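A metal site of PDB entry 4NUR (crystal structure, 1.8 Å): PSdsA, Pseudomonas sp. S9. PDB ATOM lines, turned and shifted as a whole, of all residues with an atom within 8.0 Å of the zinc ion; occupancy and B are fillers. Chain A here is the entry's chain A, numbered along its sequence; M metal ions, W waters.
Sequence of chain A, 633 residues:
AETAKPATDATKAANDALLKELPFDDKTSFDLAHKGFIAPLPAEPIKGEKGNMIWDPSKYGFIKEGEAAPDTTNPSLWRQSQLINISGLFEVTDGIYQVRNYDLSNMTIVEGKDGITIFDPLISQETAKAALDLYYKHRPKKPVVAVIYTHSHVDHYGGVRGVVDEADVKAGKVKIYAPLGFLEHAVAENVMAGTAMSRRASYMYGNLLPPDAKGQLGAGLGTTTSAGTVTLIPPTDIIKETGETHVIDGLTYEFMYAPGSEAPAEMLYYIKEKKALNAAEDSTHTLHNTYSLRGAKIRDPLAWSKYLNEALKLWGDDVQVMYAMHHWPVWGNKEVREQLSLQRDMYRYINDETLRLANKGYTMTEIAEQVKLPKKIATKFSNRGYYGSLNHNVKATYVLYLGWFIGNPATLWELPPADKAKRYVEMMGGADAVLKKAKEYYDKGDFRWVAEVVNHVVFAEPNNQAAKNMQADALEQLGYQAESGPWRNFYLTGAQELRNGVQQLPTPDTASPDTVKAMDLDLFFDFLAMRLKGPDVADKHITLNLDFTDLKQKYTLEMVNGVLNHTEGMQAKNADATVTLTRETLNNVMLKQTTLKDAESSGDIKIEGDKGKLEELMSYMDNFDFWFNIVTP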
ATOM      1  N   LEU A 104       8.086 -12.132   7.168  1.00  0.00           N
ATOM      2  CA  LEU A 104       7.050 -13.088   6.815  1.00  0.00           C
ATOM      3  C   LEU A 104       6.596 -12.881   5.375  1.00  0.00           C
ATOM      4  O   LEU A 104       6.345 -13.841   4.652  1.00  0.00           O
ATOM      5  CB  LEU A 104       5.842 -12.949   7.746  1.00  0.00           C
ATOM      6  CG  LEU A 104       4.821 -14.086   7.600  1.00  0.00           C
ATOM      7  CD1 LEU A 104       5.322 -15.384   8.262  1.00  0.00           C
ATOM      8  CD2 LEU A 104       3.476 -13.674   8.191  1.00  0.00           C
ATOM      9  N   SER A 105       6.514 -11.616   4.986  1.00  0.00           N
ATOM     10  CA  SER A 105       6.095 -11.216   3.652  1.00  0.00           C
ATOM     11  C   SER A 105       7.303 -10.849   2.774  1.00  0.00           C
ATOM     12  O   SER A 105       8.431 -10.732   3.254  1.00  0.00           O
ATOM     13  CB  SER A 105       5.201  -9.984   3.776  1.00  0.00           C
ATOM     14  OG  SER A 105       5.851  -9.044   4.634  1.00  0.00           O
ATOM     15  N   ASN A 106       7.039 -10.678   1.478  1.00  0.00           N
ATOM     16  CA  ASN A 106       8.012 -10.160   0.532  1.00  0.00           C
ATOM     17  C   ASN A 106       7.915  -8.646   0.484  1.00  0.00           C
ATOM     18  O   ASN A 106       6.862  -8.091   0.790  1.00  0.00           O
ATOM     19  CB  ASN A 106       7.667 -10.648  -0.884  1.00  0.00           C
ATOM     20  CG  ASN A 106       7.713 -12.156  -1.022  1.00  0.00           C
ATOM     21  OD1 ASN A 106       8.474 -12.834  -0.313  1.00  0.00           O
ATOM     22  ND2 ASN A 106       6.918 -12.689  -1.959  1.00  0.00           N
ATOM     23  N   ASP A 120       4.144  -3.176  -0.123  1.00  0.00           N
ATOM     24  CA  ASP A 120       4.104  -4.004   1.081  1.00  0.00           C
ATOM     25  C   ASP A 120       5.413  -4.098   1.854  1.00  0.00           C
ATOM     26  O   ASP A 120       6.062  -5.155   1.867  1.00  0.00           O
ATOM     27  CB  ASP A 120       3.611  -5.395   0.702  1.00  0.00           C
ATOM     28  CG  ASP A 120       2.169  -5.383   0.235  1.00  0.00           C
ATOM     29  OD1 ASP A 120       1.607  -4.286   0.029  1.00  0.00           O
ATOM     30  OD2 ASP A 120       1.570  -6.469   0.078  1.00  0.00           O
ATOM     31  N   ILE A 123       6.945  -6.102   8.070  1.00  0.00           N
ATOM     32  CA  ILE A 123       6.410  -5.834   9.404  1.00  0.00           C
ATOM     33  C   ILE A 123       7.149  -4.734  10.159  1.00  0.00           C
ATOM     34  O   ILE A 123       6.529  -3.917  10.849  1.00  0.00           O
ATOM     35  CB  ILE A 123       6.433  -7.120  10.267  1.00  0.00           C
ATOM     36  CG1 ILE A 123       5.435  -8.140   9.737  1.00  0.00           C
ATOM     37  CG2 ILE A 123       6.090  -6.817  11.730  1.00  0.00           C
ATOM     38  CD1 ILE A 123       5.491  -9.489  10.452  1.00  0.00           C
ATOM     39  N   THR A 150      -1.020  -3.537  -0.262  1.00  0.00           N
ATOM     40  CA  THR A 150      -2.021  -4.331  -0.982  1.00  0.00           C
ATOM     41  C   THR A 150      -3.199  -4.721  -0.095  1.00  0.00           C
ATOM     42  O   THR A 150      -4.283  -4.994  -0.597  1.00  0.00           O
ATOM     43  CB  THR A 150      -1.463  -5.605  -1.617  1.00  0.00           C
ATOM     44  OG1 THR A 150      -0.926  -6.456  -0.592  1.00  0.00           O
ATOM     45  CG2 THR A 150      -0.360  -5.274  -2.618  1.00  0.00           C
ATOM     46  N   HIS A 151      -2.976  -4.798   1.212  1.00  0.00           N
ATOM     47  CA  HIS A 151      -4.072  -5.158   2.114  1.00  0.00           C
ATOM     48  C   HIS A 151      -3.818  -4.778   3.557  1.00  0.00           C
ATOM     49  O   HIS A 151      -2.716  -4.367   3.886  1.00  0.00           O
ATOM     50  CB  HIS A 151      -4.494  -6.639   1.955  1.00  0.00           C
ATOM     51  CG  HIS A 151      -3.425  -7.653   2.242  1.00  0.00           C
ATOM     52  ND1 HIS A 151      -2.359  -7.859   1.407  1.00  0.00           N
ATOM     53  CD2 HIS A 151      -3.314  -8.562   3.238  1.00  0.00           C
ATOM     54  CE1 HIS A 151      -1.623  -8.859   1.880  1.00  0.00           C
ATOM     55  NE2 HIS A 151      -2.185  -9.307   2.976  1.00  0.00           N
ATOM     56  N   HIS A 153      -3.266  -6.024   6.522  1.00  0.00           N
ATOM     57  CA  HIS A 153      -2.544  -6.782   7.555  1.00  0.00           C
ATOM     58  C   HIS A 153      -1.126  -6.222   7.744  1.00  0.00           C
ATOM     59  O   HIS A 153      -0.514  -5.733   6.796  1.00  0.00           O
ATOM     60  CB  HIS A 153      -2.497  -8.269   7.217  1.00  0.00           C
ATOM     61  CG  HIS A 153      -3.842  -8.927   7.268  1.00  0.00           C
ATOM     62  ND1 HIS A 153      -4.201  -9.948   6.399  1.00  0.00           N
ATOM     63  CD2 HIS A 153      -4.906  -8.731   8.069  1.00  0.00           C
ATOM     64  CE1 HIS A 153      -5.436 -10.332   6.670  1.00  0.00           C
ATOM     65  NE2 HIS A 153      -5.896  -9.608   7.677  1.00  0.00           N
ATOM     66  N   VAL A 154      -0.625  -6.310   8.983  1.00  0.00           N
ATOM     67  CA  VAL A 154       0.589  -5.572   9.389  1.00  0.00           C
ATOM     68  C   VAL A 154       1.848  -5.924   8.611  1.00  0.00           C
ATOM     69  O   VAL A 154       2.753  -5.090   8.472  1.00  0.00           O
ATOM     70  CB  VAL A 154       0.839  -5.739  10.919  1.00  0.00           C
ATOM     71  CG1 VAL A 154       1.267  -7.167  11.217  1.00  0.00           C
ATOM     72  CG2 VAL A 154       1.864  -4.751  11.400  1.00  0.00           C
ATOM     73  N   ASP A 155       1.926  -7.132   8.064  1.00  0.00           N
ATOM     74  CA  ASP A 155       3.100  -7.500   7.267  1.00  0.00           C
ATOM     75  C   ASP A 155       3.110  -6.890   5.874  1.00  0.00           C
ATOM     76  O   ASP A 155       3.999  -7.170   5.062  1.00  0.00           O
ATOM     77  CB  ASP A 155       3.289  -9.031   7.182  1.00  0.00           C
ATOM     78  CG  ASP A 155       2.044  -9.764   6.784  1.00  0.00           C
ATOM     79  OD1 ASP A 155       0.920  -9.429   7.255  1.00  0.00           O
ATOM     80  OD2 ASP A 155       2.200 -10.736   6.025  1.00  0.00           O
ATOM     81  N   HIS A 156       2.147  -6.007   5.604  1.00  0.00           N
ATOM     82  CA  HIS A 156       2.080  -5.327   4.311  1.00  0.00           C
ATOM     83  C   HIS A 156       2.104  -3.819   4.430  1.00  0.00           C
ATOM     84  O   HIS A 156       1.851  -3.114   3.455  1.00  0.00           O
ATOM     85  CB  HIS A 156       0.874  -5.836   3.551  1.00  0.00           C
ATOM     86  CG  HIS A 156       0.909  -7.308   3.414  1.00  0.00           C
ATOM     87  ND1 HIS A 156       1.555  -7.940   2.360  1.00  0.00           N
ATOM     88  CD2 HIS A 156       0.516  -8.297   4.262  1.00  0.00           C
ATOM     89  CE1 HIS A 156       1.505  -9.251   2.549  1.00  0.00           C
ATOM     90  NE2 HIS A 156       0.893  -9.478   3.678  1.00  0.00           N
ATOM     91  N   TYR A 205       2.507 -18.621  15.406  1.00  0.00           N
ATOM     92  CA  TYR A 205       3.741 -18.387  14.660  1.00  0.00           C
ATOM     93  C   TYR A 205       4.940 -19.084  15.271  1.00  0.00           C
ATOM     94  O   TYR A 205       6.068 -18.927  14.802  1.00  0.00           O
ATOM     95  CB  TYR A 205       4.002 -16.889  14.501  1.00  0.00           C
ATOM     96  CG  TYR A 205       3.100 -16.309  13.450  1.00  0.00           C
ATOM     97  CD1 TYR A 205       3.311 -16.606  12.115  1.00  0.00           C
ATOM     98  CD2 TYR A 205       2.005 -15.529  13.801  1.00  0.00           C
ATOM     99  CE1 TYR A 205       2.460 -16.095  11.125  1.00  0.00           C
ATOM    100  CE2 TYR A 205       1.154 -15.014  12.827  1.00  0.00           C
ATOM    101  CZ  TYR A 205       1.389 -15.305  11.492  1.00  0.00           C
ATOM    102  OH  TYR A 205       0.546 -14.812  10.513  1.00  0.00           O
ATOM    103  N   LEU A 221       3.619 -20.039   5.058  1.00  0.00           N
ATOM    104  CA  LEU A 221       3.423 -18.881   4.186  1.00  0.00           C
ATOM    105  C   LEU A 221       4.713 -18.059   4.143  1.00  0.00           C
ATOM    106  O   LEU A 221       5.006 -17.352   3.180  1.00  0.00           O
ATOM    107  CB  LEU A 221       2.288 -18.050   4.748  1.00  0.00           C
ATOM    108  CG  LEU A 221       1.977 -16.761   4.010  1.00  0.00           C
ATOM    109  CD1 LEU A 221       1.153 -17.046   2.755  1.00  0.00           C
ATOM    110  CD2 LEU A 221       1.215 -15.883   4.958  1.00  0.00           C
ATOM    111  N   GLU A 262      -8.708 -12.574   1.404  1.00  0.00           N
ATOM    112  CA  GLU A 262      -7.700 -12.875   2.432  1.00  0.00           C
ATOM    113  C   GLU A 262      -7.716 -11.838   3.567  1.00  0.00           C
ATOM    114  O   GLU A 262      -7.377 -12.151   4.724  1.00  0.00           O
ATOM    115  CB  GLU A 262      -6.316 -13.006   1.771  1.00  0.00           C
ATOM    116  CG  GLU A 262      -5.215 -13.438   2.706  1.00  0.00           C
ATOM    117  CD  GLU A 262      -4.599 -12.283   3.454  1.00  0.00           C
ATOM    118  OE1 GLU A 262      -4.753 -11.138   2.994  1.00  0.00           O
ATOM    119  OE2 GLU A 262      -3.978 -12.509   4.512  1.00  0.00           O
ATOM    120  N   GLU A 266      -8.483  -5.488   0.516  1.00  0.00           N
ATOM    121  CA  GLU A 266      -7.403  -6.087  -0.278  1.00  0.00           C
ATOM    122  C   GLU A 266      -7.626  -5.724  -1.732  1.00  0.00           C
ATOM    123  O   GLU A 266      -8.761  -5.543  -2.152  1.00  0.00           O
ATOM    124  CB  GLU A 266      -7.396  -7.611  -0.111  1.00  0.00           C
ATOM    125  CG  GLU A 266      -6.255  -8.345  -0.847  1.00  0.00           C
ATOM    126  CD  GLU A 266      -5.674  -9.493  -0.026  1.00  0.00           C
ATOM    127  OE1 GLU A 266      -6.046  -9.670   1.158  1.00  0.00           O
ATOM    128  OE2 GLU A 266      -4.816 -10.234  -0.555  1.00  0.00           O
ATOM    129  N   ALA A 280      -1.483 -10.213  -4.755  1.00  0.00           N
ATOM    130  CA  ALA A 280      -1.623  -9.757  -3.367  1.00  0.00           C
ATOM    131  C   ALA A 280      -1.377 -10.939  -2.436  1.00  0.00           C
ATOM    132  O   ALA A 280      -0.312 -11.539  -2.487  1.00  0.00           O
ATOM    133  CB  ALA A 280      -2.997  -9.138  -3.131  1.00  0.00           C
ATOM    134  N   GLU A 281      -2.349 -11.295  -1.600  1.00  0.00           N
ATOM    135  CA  GLU A 281      -2.217 -12.547  -0.843  1.00  0.00           C
ATOM    136  C   GLU A 281      -3.348 -13.509  -1.176  1.00  0.00           C
ATOM    137  O   GLU A 281      -3.633 -14.452  -0.438  1.00  0.00           O
ATOM    138  CB  GLU A 281      -2.144 -12.257   0.669  1.00  0.00           C
ATOM    139  CG  GLU A 281      -1.573 -13.414   1.493  1.00  0.00           C
ATOM    140  CD  GLU A 281      -1.082 -13.010   2.860  1.00  0.00           C
ATOM    141  OE1 GLU A 281      -0.758 -11.803   3.053  1.00  0.00           O
ATOM    142  OE2 GLU A 281      -1.005 -13.891   3.748  1.00  0.00           O
ATOM    143  N   THR A 284      -1.239 -17.601  -3.642  1.00  0.00           N
ATOM    144  CA  THR A 284       0.148 -17.849  -3.239  1.00  0.00           C
ATOM    145  C   THR A 284       0.363 -19.344  -3.376  1.00  0.00           C
ATOM    146  O   THR A 284      -0.498 -20.057  -3.882  1.00  0.00           O
ATOM    147  CB  THR A 284       0.427 -17.427  -1.777  1.00  0.00           C
ATOM    148  OG1 THR A 284      -0.463 -18.125  -0.905  1.00  0.00           O
ATOM    149  CG2 THR A 284       0.220 -15.930  -1.592  1.00  0.00           C
ATOM    150  N   HIS A 288      -4.734 -21.046   1.682  1.00  0.00           N
ATOM    151  CA  HIS A 288      -4.629 -19.985   2.674  1.00  0.00           C
ATOM    152  C   HIS A 288      -5.784 -20.125   3.668  1.00  0.00           C
ATOM    153  O   HIS A 288      -6.527 -21.093   3.616  1.00  0.00           O
ATOM    154  CB  HIS A 288      -4.676 -18.623   1.973  1.00  0.00           C
ATOM    155  CG  HIS A 288      -3.982 -17.529   2.715  1.00  0.00           C
ATOM    156  ND1 HIS A 288      -4.487 -16.953   3.855  1.00  0.00           N
ATOM    157  CD2 HIS A 288      -2.812 -16.890   2.453  1.00  0.00           C
ATOM    158  CE1 HIS A 288      -3.669 -16.011   4.276  1.00  0.00           C
ATOM    159  NE2 HIS A 288      -2.643 -15.958   3.451  1.00  0.00           N
ATOM    160  N   MET A 325       2.640 -11.365  -2.617  1.00  0.00           N
ATOM    161  CA  MET A 325       3.283 -10.676  -1.496  1.00  0.00           C
ATOM    162  C   MET A 325       3.839 -11.661  -0.478  1.00  0.00           C
ATOM    163  O   MET A 325       4.426 -11.249   0.542  1.00  0.00           O
ATOM    164  CB  MET A 325       2.311  -9.644  -0.906  1.00  0.00           C
ATOM    165  CG  MET A 325       1.667  -8.734  -1.986  1.00  0.00           C
ATOM    166  SD  MET A 325       2.808  -7.497  -2.678  1.00  0.00           S
ATOM    167  CE  MET A 325       3.510  -8.356  -4.101  1.00  0.00           C
ATOM    168  N   HIS A 326       3.640 -12.945  -0.755  1.00  0.00           N
ATOM    169  CA  HIS A 326       4.368 -14.051  -0.111  1.00  0.00           C
ATOM    170  C   HIS A 326       4.744 -15.034  -1.191  1.00  0.00           C
ATOM    171  O   HIS A 326       4.103 -15.081  -2.241  1.00  0.00           O
ATOM    172  CB  HIS A 326       3.495 -14.793   0.896  1.00  0.00           C
ATOM    173  CG  HIS A 326       3.099 -13.956   2.055  1.00  0.00           C
ATOM    174  ND1 HIS A 326       3.862 -13.877   3.200  1.00  0.00           N
ATOM    175  CD2 HIS A 326       2.048 -13.123   2.235  1.00  0.00           C
ATOM    176  CE1 HIS A 326       3.277 -13.053   4.054  1.00  0.00           C
ATOM    177  NE2 HIS A 326       2.195 -12.581   3.495  1.00  0.00           N
ATOM    178  N   TYR A 387      -0.531 -23.223   5.351  1.00  0.00           N
ATOM    179  CA  TYR A 387      -0.859 -22.103   6.211  1.00  0.00           C
ATOM    180  C   TYR A 387      -2.304 -22.302   6.654  1.00  0.00           C
ATOM    181  O   TYR A 387      -2.581 -22.599   7.802  1.00  0.00           O
ATOM    182  CB  TYR A 387      -0.611 -20.799   5.470  1.00  0.00           C
ATOM    183  CG  TYR A 387      -0.734 -19.537   6.312  1.00  0.00           C
ATOM    184  CD1 TYR A 387       0.124 -19.311   7.382  1.00  0.00           C
ATOM    185  CD2 TYR A 387      -1.687 -18.584   6.021  1.00  0.00           C
ATOM    186  CE1 TYR A 387       0.018 -18.155   8.143  1.00  0.00           C
ATOM    187  CE2 TYR A 387      -1.789 -17.424   6.769  1.00  0.00           C
ATOM    188  CZ  TYR A 387      -0.927 -17.216   7.826  1.00  0.00           C
ATOM    189  OH  TYR A 387      -1.046 -16.061   8.568  1.00  0.00           O
HETATM  190 ZN    ZN M   1       0.735 -11.371   4.580  1.00  0.00          ZN
HETATM  191  O   HOH W   1       0.325 -13.158   5.953  1.00  0.00           O
HETATM  192  O   HOH W   2      -0.917 -10.836   5.923  1.00  0.00           O
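The side-chain carboxylate of Glu 281 lies close to a ring nitrogen (NE2) of His 151, 2.9 Å away.
A ring nitrogen (ND1) of His 156 sits at hydrogen-bond distance from the side-chain carboxylate (OD2) of Asp 120, at 2.7 Å.
A ring nitrogen (NE2) of His 288 is in hydrogen-bond range of the side-chain carboxylate of Glu 281 (2.7 Å).
The side-chain carboxylate (OE1) of Glu 262 sits close to a ring nitrogen (NE2) of His 151.
OG1 of Thr 150 is in hydrogen-bond range of ND1 of His 151.
OG of Ser 105 is in hydrogen-bond range of O of Asp 155.
A ring nitrogen (NE2) of His 151 lies close to a ring nitrogen (NE2) of His 156 (3.2 Å).
The backbone NH (N) of Glu 281 lies within hydrogen-bond range of the side-chain carboxylate (OE2) of Glu 266, at 2.9 Å.
His 151 touches the zinc ion.
Five residues have an atom within 4 Å of the zinc ion: His 151, Asp 155, His 156, Glu 281 and His 326.
The nearest printed residue that does not touch the zinc ion is Leu 221 (4.6 Å).
The zinc ion is bound by NE2 of His 156 (2.1 Å), OD2 of Asp 155 (2.2 Å), OE1 of Glu 281 (2.2 Å), NE2 of His 326 (2.2 Å), water W2 (2.2 Å) and water W1 (2.3 Å).
The zinc ion has six donor atoms within binding distance.
Water W2 bridges the side-chain carboxylate of Asp 155 (2.7 Å) and a ring nitrogen (ND1) of His 153 (3.4 Å).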
